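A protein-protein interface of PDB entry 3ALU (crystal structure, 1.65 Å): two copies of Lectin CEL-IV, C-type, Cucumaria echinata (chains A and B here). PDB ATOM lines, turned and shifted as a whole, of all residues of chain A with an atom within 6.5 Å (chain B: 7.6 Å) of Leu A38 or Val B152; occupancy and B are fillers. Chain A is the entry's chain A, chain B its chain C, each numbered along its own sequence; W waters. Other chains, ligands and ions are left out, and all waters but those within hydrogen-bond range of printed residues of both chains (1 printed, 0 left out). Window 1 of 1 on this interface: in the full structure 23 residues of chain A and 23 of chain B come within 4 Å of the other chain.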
ATOM      1  N   PHE A  36      24.774 -19.734  40.271  1.00  0.00           N
ATOM      2  CA  PHE A  36      25.431 -19.141  39.130  1.00  0.00           C
ATOM      3  C   PHE A  36      25.703 -20.224  38.104  1.00  0.00           C
ATOM      4  O   PHE A  36      26.081 -21.352  38.446  1.00  0.00           O
ATOM      5  CB  PHE A  36      26.724 -18.409  39.563  1.00  0.00           C
ATOM      6  CG  PHE A  36      26.477 -17.415  40.680  1.00  0.00           C
ATOM      7  CD1 PHE A  36      25.877 -16.183  40.422  1.00  0.00           C
ATOM      8  CD2 PHE A  36      26.817 -17.732  42.000  1.00  0.00           C
ATOM      9  CE1 PHE A  36      25.617 -15.284  41.440  1.00  0.00           C
ATOM     10  CE2 PHE A  36      26.543 -16.850  43.041  1.00  0.00           C
ATOM     11  CZ  PHE A  36      25.957 -15.599  42.762  1.00  0.00           C
ATOM     12  N   GLY A  37      25.411 -19.913  36.844  1.00  0.00           N
ATOM     13  CA  GLY A  37      25.527 -20.926  35.803  1.00  0.00           C
ATOM     14  C   GLY A  37      26.298 -20.474  34.578  1.00  0.00           C
ATOM     15  O   GLY A  37      26.654 -19.289  34.419  1.00  0.00           O
ATOM     16  N   LEU A  38      26.558 -21.448  33.714  1.00  0.00           N
ATOM     17  CA  LEU A  38      27.078 -21.209  32.377  1.00  0.00           C
ATOM     18  C   LEU A  38      26.108 -21.882  31.430  1.00  0.00           C
ATOM     19  O   LEU A  38      25.808 -23.083  31.556  1.00  0.00           O
ATOM     20  CB  LEU A  38      28.467 -21.810  32.261  1.00  0.00           C
ATOM     21  CG  LEU A  38      29.559 -21.359  31.294  1.00  0.00           C
ATOM     22  CD1 LEU A  38      29.992 -22.444  30.327  1.00  0.00           C
ATOM     23  CD2 LEU A  38      29.413 -20.006  30.663  1.00  0.00           C
ATOM     24  N   ALA A  39      25.573 -21.112  30.488  1.00  0.00           N
ATOM     25  CA  ALA A  39      24.573 -21.659  29.609  1.00  0.00           C
ATOM     26  C   ALA A  39      25.060 -21.479  28.183  1.00  0.00           C
ATOM     27  O   ALA A  39      25.793 -20.532  27.894  1.00  0.00           O
ATOM     28  CB  ALA A  39      23.247 -20.936  29.804  1.00  0.00           C
ATOM     29  N   SER A  40      24.659 -22.380  27.299  1.00  0.00           N
ATOM     30  CA  SER A  40      24.868 -22.138  25.875  1.00  0.00           C
ATOM     31  C   SER A  40      23.922 -21.011  25.447  1.00  0.00           C
ATOM     32  O   SER A  40      22.881 -20.735  26.096  1.00  0.00           O
ATOM     33  CB  SER A  40      24.584 -23.412  25.076  1.00  0.00           C
ATOM     34  OG  SER A  40      23.176 -23.525  24.875  1.00  0.00           O
ATOM     35  N   CYS A  41      24.278 -20.323  24.367  1.00  0.00           N
ATOM     36  CA  CYS A  41      23.432 -19.228  23.901  1.00  0.00           C
ATOM     37  C   CYS A  41      22.071 -19.708  23.394  1.00  0.00           C
ATOM     38  O   CYS A  41      21.093 -18.947  23.448  1.00  0.00           O
ATOM     39  CB  CYS A  41      24.154 -18.412  22.843  1.00  0.00           C
ATOM     40  SG  CYS A  41      25.615 -17.604  23.506  1.00  0.00           S
ATOM     41  N   ASP A  44      20.874 -23.972  26.838  1.00  0.00           N
ATOM     42  CA  ASP A  44      21.110 -25.202  27.606  1.00  0.00           C
ATOM     43  C   ASP A  44      22.101 -24.926  28.746  1.00  0.00           C
ATOM     44  O   ASP A  44      23.168 -24.382  28.491  1.00  0.00           O
ATOM     45  CB  ASP A  44      21.684 -26.309  26.700  1.00  0.00           C
ATOM     46  CG  ASP A  44      20.759 -26.674  25.525  1.00  0.00           C
ATOM     47  OD1 ASP A  44      19.539 -26.811  25.726  1.00  0.00           O
ATOM     48  OD2 ASP A  44      21.275 -26.863  24.401  1.00  0.00           O
ATOM     49  N   GLU A  45      21.764 -25.280  29.990  1.00  0.00           N
ATOM     50  CA  GLU A  45      22.749 -25.155  31.095  1.00  0.00           C
ATOM     51  C   GLU A  45      23.852 -26.193  30.942  1.00  0.00           C
ATOM     52  O   GLU A  45      23.577 -27.390  30.801  1.00  0.00           O
ATOM     53  CB  GLU A  45      22.113 -25.279  32.493  1.00  0.00           C
ATOM     54  CG  GLU A  45      23.167 -25.029  33.607  1.00  0.00           C
ATOM     55  CD  GLU A  45      22.565 -24.691  34.954  1.00  0.00           C
ATOM     56  OE1 GLU A  45      22.100 -25.629  35.637  1.00  0.00           O
ATOM     57  OE2 GLU A  45      22.558 -23.487  35.320  1.00  0.00           O
ATOM     58  N   LEU A  46      25.097 -25.722  30.965  1.00  0.00           N
ATOM     59  CA  LEU A  46      26.249 -26.559  30.721  1.00  0.00           C
ATOM     60  C   LEU A  46      26.993 -26.872  32.001  1.00  0.00           C
ATOM     61  O   LEU A  46      27.558 -27.985  32.185  1.00  0.00           O
ATOM     62  CB  LEU A  46      27.203 -25.851  29.765  1.00  0.00           C
ATOM     63  CG  LEU A  46      26.658 -25.522  28.381  1.00  0.00           C
ATOM     64  CD1 LEU A  46      27.796 -24.931  27.554  1.00  0.00           C
ATOM     65  CD2 LEU A  46      26.048 -26.761  27.755  1.00  0.00           C
ATOM     66  N   ALA A  47      27.031 -25.882  32.882  1.00  0.00           N
ATOM     67  CA  ALA A  47      27.806 -26.005  34.133  1.00  0.00           C
ATOM     68  C   ALA A  47      27.282 -25.074  35.212  1.00  0.00           C
ATOM     69  O   ALA A  47      26.543 -24.168  34.913  1.00  0.00           O
ATOM     70  CB  ALA A  47      29.293 -25.733  33.852  1.00  0.00           C
ATOM     71  N   THR A  48      27.624 -25.319  36.484  1.00  0.00           N
ATOM     72  CA  THR A  48      27.306 -24.355  37.569  1.00  0.00           C
ATOM     73  C   THR A  48      28.567 -23.846  38.212  1.00  0.00           C
ATOM     74  O   THR A  48      29.643 -24.452  38.071  1.00  0.00           O
ATOM     75  CB  THR A  48      26.543 -24.984  38.625  1.00  0.00           C
ATOM     76  OG1 THR A  48      27.136 -26.072  39.171  1.00  0.00           O
ATOM     77  CG2 THR A  48      25.232 -25.242  38.192  1.00  0.00           C
ATOM     78  N   GLY A  49      28.425 -22.750  38.926  1.00  0.00           N
ATOM     79  CA  GLY A  49      29.475 -22.321  39.858  1.00  0.00           C
ATOM     80  C   GLY A  49      29.588 -23.318  41.012  1.00  0.00           C
ATOM     81  O   GLY A  49      28.773 -24.255  41.160  1.00  0.00           O
ATOM     82  N   PRO A 150      31.763 -21.076  36.684  1.00  0.00           N
ATOM     83  CA  PRO A 150      32.223 -22.220  35.957  1.00  0.00           C
ATOM     84  C   PRO A 150      33.524 -21.898  35.218  1.00  0.00           C
ATOM     85  O   PRO A 150      33.607 -20.867  34.532  1.00  0.00           O
ATOM     86  CB  PRO A 150      31.062 -22.512  34.965  1.00  0.00           C
ATOM     87  CG  PRO A 150      29.880 -21.927  35.585  1.00  0.00           C
ATOM     88  CD  PRO A 150      30.337 -20.783  36.438  1.00  0.00           C
ATOM     89  N   VAL A 152      36.068 -22.634  32.406  1.00  0.00           N
ATOM     90  CA  VAL A 152      36.029 -23.291  31.097  1.00  0.00           C
ATOM     91  C   VAL A 152      37.080 -22.711  30.189  1.00  0.00           C
ATOM     92  O   VAL A 152      37.513 -21.582  30.372  1.00  0.00           O
ATOM     93  CB  VAL A 152      34.660 -23.135  30.414  1.00  0.00           C
ATOM     94  CG1 VAL A 152      33.585 -23.837  31.247  1.00  0.00           C
ATOM     95  CG2 VAL A 152      34.300 -21.649  30.221  1.00  0.00           C
ATOM     96  N   TYR A 154      38.506 -22.974  25.805  1.00  0.00           N
ATOM     97  CA  TYR A 154      38.323 -23.510  24.454  1.00  0.00           C
ATOM     98  C   TYR A 154      39.325 -24.608  24.187  1.00  0.00           C
ATOM     99  O   TYR A 154      40.455 -24.561  24.669  1.00  0.00           O
ATOM    100  CB  TYR A 154      38.489 -22.420  23.412  1.00  0.00           C
ATOM    101  CG  TYR A 154      37.432 -21.361  23.472  1.00  0.00           C
ATOM    102  CD1 TYR A 154      36.101 -21.660  23.235  1.00  0.00           C
ATOM    103  CD2 TYR A 154      37.766 -20.036  23.755  1.00  0.00           C
ATOM    104  CE1 TYR A 154      35.139 -20.679  23.306  1.00  0.00           C
ATOM    105  CE2 TYR A 154      36.839 -19.073  23.775  1.00  0.00           C
ATOM    106  CZ  TYR A 154      35.521 -19.383  23.556  1.00  0.00           C
ATOM    107  OH  TYR A 154      34.579 -18.391  23.598  1.00  0.00           O
ATOM    108  N   GLY B  14      30.182 -10.972  21.744  1.00  0.00           N
ATOM    109  CA  GLY B  14      30.356 -12.093  22.656  1.00  0.00           C
ATOM    110  C   GLY B  14      30.580 -13.450  22.000  1.00  0.00           C
ATOM    111  O   GLY B  14      30.590 -14.471  22.691  1.00  0.00           O
ATOM    112  N   LYS B  15      30.740 -13.472  20.674  1.00  0.00           N
ATOM    113  CA  LYS B  15      30.946 -14.741  19.954  1.00  0.00           C
ATOM    114  C   LYS B  15      32.249 -14.673  19.185  1.00  0.00           C
ATOM    115  O   LYS B  15      32.655 -13.580  18.787  1.00  0.00           O
ATOM    116  CB  LYS B  15      29.804 -14.966  18.976  1.00  0.00           C
ATOM    117  CG  LYS B  15      28.556 -15.401  19.681  1.00  0.00           C
ATOM    118  CD  LYS B  15      27.383 -15.609  18.708  1.00  0.00           C
ATOM    119  CE  LYS B  15      27.535 -16.907  17.916  1.00  0.00           C
ATOM    120  NZ  LYS B  15      26.318 -17.116  17.052  1.00  0.00           N
ATOM    121  N   LEU B  38      34.644 -26.562  23.844  1.00  0.00           N
ATOM    122  CA  LEU B  38      34.706 -25.908  25.135  1.00  0.00           C
ATOM    123  C   LEU B  38      34.740 -26.992  26.179  1.00  0.00           C
ATOM    124  O   LEU B  38      33.916 -27.921  26.149  1.00  0.00           O
ATOM    125  CB  LEU B  38      33.436 -25.078  25.307  1.00  0.00           C
ATOM    126  CG  LEU B  38      33.306 -23.793  26.170  1.00  0.00           C
ATOM    127  CD1 LEU B  38      32.156 -23.840  27.184  1.00  0.00           C
ATOM    128  CD2 LEU B  38      34.568 -23.222  26.726  1.00  0.00           C
ATOM    129  N   ALA B  39      35.710 -26.904  27.083  1.00  0.00           N
ATOM    130  CA  ALA B  39      35.839 -27.895  28.148  1.00  0.00           C
ATOM    131  C   ALA B  39      35.902 -27.227  29.524  1.00  0.00           C
ATOM    132  O   ALA B  39      36.326 -26.079  29.640  1.00  0.00           O
ATOM    133  CB  ALA B  39      37.089 -28.728  27.928  1.00  0.00           C
ATOM    134  N   LEU B  46      32.239 -29.849  27.246  1.00  0.00           N
ATOM    135  CA  LEU B  46      30.954 -29.251  27.553  1.00  0.00           C
ATOM    136  C   LEU B  46      30.170 -28.910  26.297  1.00  0.00           C
ATOM    137  O   LEU B  46      28.957 -29.044  26.277  1.00  0.00           O
ATOM    138  CB  LEU B  46      31.135 -27.956  28.362  1.00  0.00           C
ATOM    139  CG  LEU B  46      31.717 -28.111  29.784  1.00  0.00           C
ATOM    140  CD1 LEU B  46      31.804 -26.771  30.457  1.00  0.00           C
ATOM    141  CD2 LEU B  46      30.890 -29.083  30.658  1.00  0.00           C
ATOM    142  N   ALA B  47      30.868 -28.444  25.266  1.00  0.00           N
ATOM    143  CA  ALA B  47      30.181 -28.003  24.056  1.00  0.00           C
ATOM    144  C   ALA B  47      31.133 -28.074  22.890  1.00  0.00           C
ATOM    145  O   ALA B  47      32.347 -28.217  23.057  1.00  0.00           O
ATOM    146  CB  ALA B  47      29.630 -26.579  24.229  1.00  0.00           C
ATOM    147  N   LEU B 149      33.058 -20.564  17.696  1.00  0.00           N
ATOM    148  CA  LEU B 149      33.350 -21.330  18.900  1.00  0.00           C
ATOM    149  C   LEU B 149      32.055 -21.460  19.726  1.00  0.00           C
ATOM    150  O   LEU B 149      31.109 -20.706  19.525  1.00  0.00           O
ATOM    151  CB  LEU B 149      34.471 -20.658  19.715  1.00  0.00           C
ATOM    152  CG  LEU B 149      35.856 -20.679  19.062  1.00  0.00           C
ATOM    153  CD1 LEU B 149      36.858 -19.903  19.909  1.00  0.00           C
ATOM    154  CD2 LEU B 149      36.331 -22.120  18.855  1.00  0.00           C
ATOM    155  N   PRO B 150      32.006 -22.425  20.662  1.00  0.00           N
ATOM    156  CA  PRO B 150      30.777 -22.565  21.471  1.00  0.00           C
ATOM    157  C   PRO B 150      30.389 -21.238  22.112  1.00  0.00           C
ATOM    158  O   PRO B 150      31.233 -20.561  22.721  1.00  0.00           O
ATOM    159  CB  PRO B 150      31.193 -23.574  22.550  1.00  0.00           C
ATOM    160  CG  PRO B 150      32.182 -24.432  21.843  1.00  0.00           C
ATOM    161  CD  PRO B 150      32.989 -23.466  20.967  1.00  0.00           C
ATOM    162  N   CYS B 151      29.123 -20.849  21.910  1.00  0.00           N
ATOM    163  CA  CYS B 151      28.604 -19.571  22.378  1.00  0.00           C
ATOM    164  C   CYS B 151      28.026 -19.808  23.758  1.00  0.00           C
ATOM    165  O   CYS B 151      27.072 -20.567  23.898  1.00  0.00           O
ATOM    166  CB  CYS B 151      27.456 -19.132  21.470  1.00  0.00           C
ATOM    167  SG  CYS B 151      26.826 -17.481  21.838  1.00  0.00           S
ATOM    168  N   VAL B 152      28.601 -19.177  24.765  1.00  0.00           N
ATOM    169  CA  VAL B 152      28.127 -19.400  26.145  1.00  0.00           C
ATOM    170  C   VAL B 152      28.104 -18.087  26.896  1.00  0.00           C
ATOM    171  O   VAL B 152      28.783 -17.105  26.526  1.00  0.00           O
ATOM    172  CB  VAL B 152      29.034 -20.379  26.946  1.00  0.00           C
ATOM    173  CG1 VAL B 152      29.074 -21.748  26.294  1.00  0.00           C
ATOM    174  CG2 VAL B 152      30.466 -19.823  27.108  1.00  0.00           C
ATOM    175  N   HIS B 153      27.335 -18.062  27.969  1.00  0.00           N
ATOM    176  CA  HIS B 153      27.275 -16.871  28.771  1.00  0.00           C
ATOM    177  C   HIS B 153      26.960 -17.311  30.193  1.00  0.00           C
ATOM    178  O   HIS B 153      26.413 -18.404  30.410  1.00  0.00           O
ATOM    179  CB  HIS B 153      26.192 -15.923  28.242  1.00  0.00           C
ATOM    180  CG  HIS B 153      24.795 -16.425  28.400  1.00  0.00           C
ATOM    181  ND1 HIS B 153      24.216 -17.324  27.524  1.00  0.00           N
ATOM    182  CD2 HIS B 153      23.837 -16.114  29.308  1.00  0.00           C
ATOM    183  CE1 HIS B 153      22.970 -17.564  27.903  1.00  0.00           C
ATOM    184  NE2 HIS B 153      22.716 -16.839  28.980  1.00  0.00           N
ATOM    185  N   TYR B 154      27.346 -16.479  31.146  1.00  0.00           N
ATOM    186  CA  TYR B 154      26.969 -16.712  32.545  1.00  0.00           C
ATOM    187  C   TYR B 154      25.528 -16.359  32.857  1.00  0.00           C
ATOM    188  O   TYR B 154      24.965 -15.375  32.340  1.00  0.00           O
ATOM    189  CB  TYR B 154      27.889 -15.939  33.483  1.00  0.00           C
ATOM    190  CG  TYR B 154      29.355 -16.264  33.397  1.00  0.00           C
ATOM    191  CD1 TYR B 154      29.825 -17.540  33.673  1.00  0.00           C
ATOM    192  CD2 TYR B 154      30.285 -15.277  33.072  1.00  0.00           C
ATOM    193  CE1 TYR B 154      31.170 -17.841  33.603  1.00  0.00           C
ATOM    194  CE2 TYR B 154      31.640 -15.560  33.015  1.00  0.00           C
ATOM    195  CZ  TYR B 154      32.074 -16.839  33.271  1.00  0.00           C
ATOM    196  OH  TYR B 154      33.406 -17.116  33.236  1.00  0.00           O
ATOM    197  N   THR B 155      24.922 -17.143  33.749  1.00  0.00           N
ATOM    198  CA  THR B 155      23.562 -16.880  34.193  1.00  0.00           C
ATOM    199  C   THR B 155      23.662 -16.540  35.679  1.00  0.00           C
ATOM    200  O   THR B 155      24.029 -17.382  36.501  1.00  0.00           O
ATOM    201  CB  THR B 155      22.645 -18.095  33.968  1.00  0.00           C
ATOM    202  OG1 THR B 155      23.304 -19.260  34.483  1.00  0.00           O
ATOM    203  CG2 THR B 155      22.368 -18.306  32.468  1.00  0.00           C
ATOM    204  N   LEU B 156      23.386 -15.287  36.016  1.00  0.00           N
ATOM    205  CA  LEU B 156      23.752 -14.774  37.332  1.00  0.00           C
ATOM    206  C   LEU B 156      22.544 -14.536  38.232  1.00  0.00           C
ATOM    207  O   LEU B 156      22.324 -13.422  38.721  1.00  0.00           O
ATOM    208  CB  LEU B 156      24.640 -13.522  37.203  1.00  0.00           C
ATOM    209  CG  LEU B 156      25.960 -13.788  36.462  1.00  0.00           C
ATOM    210  CD1 LEU B 156      26.753 -12.506  36.307  1.00  0.00           C
ATOM    211  CD2 LEU B 156      26.798 -14.839  37.193  1.00  0.00           C
HETATM  212  O   HOH W   1      22.569 -21.879  33.375  1.00  0.00           O
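O of Gly A37 lies within hydrogen-bond range of N of Thr B155, 2.8 Å away. The backbone carbonyl oxygen (O) of His B153 sits at hydrogen-bond distance from the backbone NH (N) of Ala A39 (2.8 Å). The side-chain sulfur (SG) of Cys A41 is disulfide-bonded to the side-chain sulfur (SG) of Cys B151. The backbone NH of Val B152 lies within hydrogen-bond range of the side-chain sulfur of Cys A41, at 3.6 Å.
Leu A38 touches Val B152, and with the chains exchanged Val A152 touches Leu B38. Ala A39 touches Val B152, and with the chains exchanged Val A152 touches Ala B39. Leu B46 touches its own counterpart, Leu A46. Leu A46 touches Val B152, and with the chains exchanged Val A152 touches Leu B46. Positions printed for both chains: 38, 39, 46, 47, 150, 152 and 154.
The backbone carbonyl oxygen of Phe A36 lies within hydrogen-bond range of the backbone NH of Gly A49 (2.8 Å). The backbone carbonyl oxygen of Leu A38 lies within hydrogen-bond range of the backbone NH of Leu A46, 2.8 Å away. The backbone NH (N) of Leu A38 is in hydrogen-bond range of the backbone carbonyl oxygen (O) of Ala A47. OG of Ser A40 sits at hydrogen-bond distance from N of Asp A44 (3.1 Å). O of Leu B38 sits at hydrogen-bond distance from N of Leu B46, at 2.8 Å. The backbone NH of Leu B38 lies within hydrogen-bond range of the backbone carbonyl oxygen of Ala B47, 2.9 Å away.
Of chain A, only Leu A38, Ala A39, Cys A41 and Leu A46 come within 4 Å of Val B152. Ala A39 touches three residues of chain B. Printed residues of chain B within 4 Å of Cys A41: Cys B151 and Val B152. Of the printed residues of chain A, Thr B155 touches Phe A36, Gly A37, Leu A38 and Ala A39. Of the printed residues of chain A, His B153 touches Leu A38, Ala A39 and Ser A40. Glu A45 touches none of the printed residues of chain B. Ala B47 touches none of the printed residues of chain A. The nearest residue of chain A that does not touch Val B152 is Ser A40 (4.2 Å).
Thr B155 touches Phe A36 (O to CA, 3.5 Å). Phe A36 touches Leu B156 (CD1 to CD2, 3.6 Å). Leu A38 touches His B153. Leu A38 touches Tyr B154. Thr B155 touches Leu A38. Val B152 touches Ala A39. Cys B151 touches Ser A40. Leu B46 touches Leu A46. Tyr B154 touches Pro A150 (OH to O, 3.97 Å). Pro B150 touches Tyr A154.
Water W1 lies within hydrogen-bond range of the side-chain carboxylate of Glu A45 (2.5 Å) and the side-chain hydroxyl of Thr B155 (2.9 Å).
Of the 14 printed residues of chain B, 11 touch a printed residue of chain A. Hydrophobic or aromatic side chains of chain B within 4 Å of the printed part of chain A: Leu B38, Leu B46, Leu B149, Val B152, His B153, Tyr B154 and Leu B156. Of the 15 printed residues of chain A, 10 touch a printed residue of chain B. Printed residues of chain A that touch a printed residue of chain B: Phe A36, Gly A37, Leu A38, Ala A39, Ser A40, Cys A41, Leu A46, Pro A150, Val A152 and Tyr A154. Hydrophobic or aromatic side chains of chain A that line the printed part of chain B: Phe A36, Leu A38, Ala A39, Leu A46, Val A152 and Tyr A154. Among the printed residues, 23 pairs touch across the chains. Among the printed residues, no Asp or Glu carboxylate lies within 4 Å of a Lys or Arg side-chain nitrogen of the other chain.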
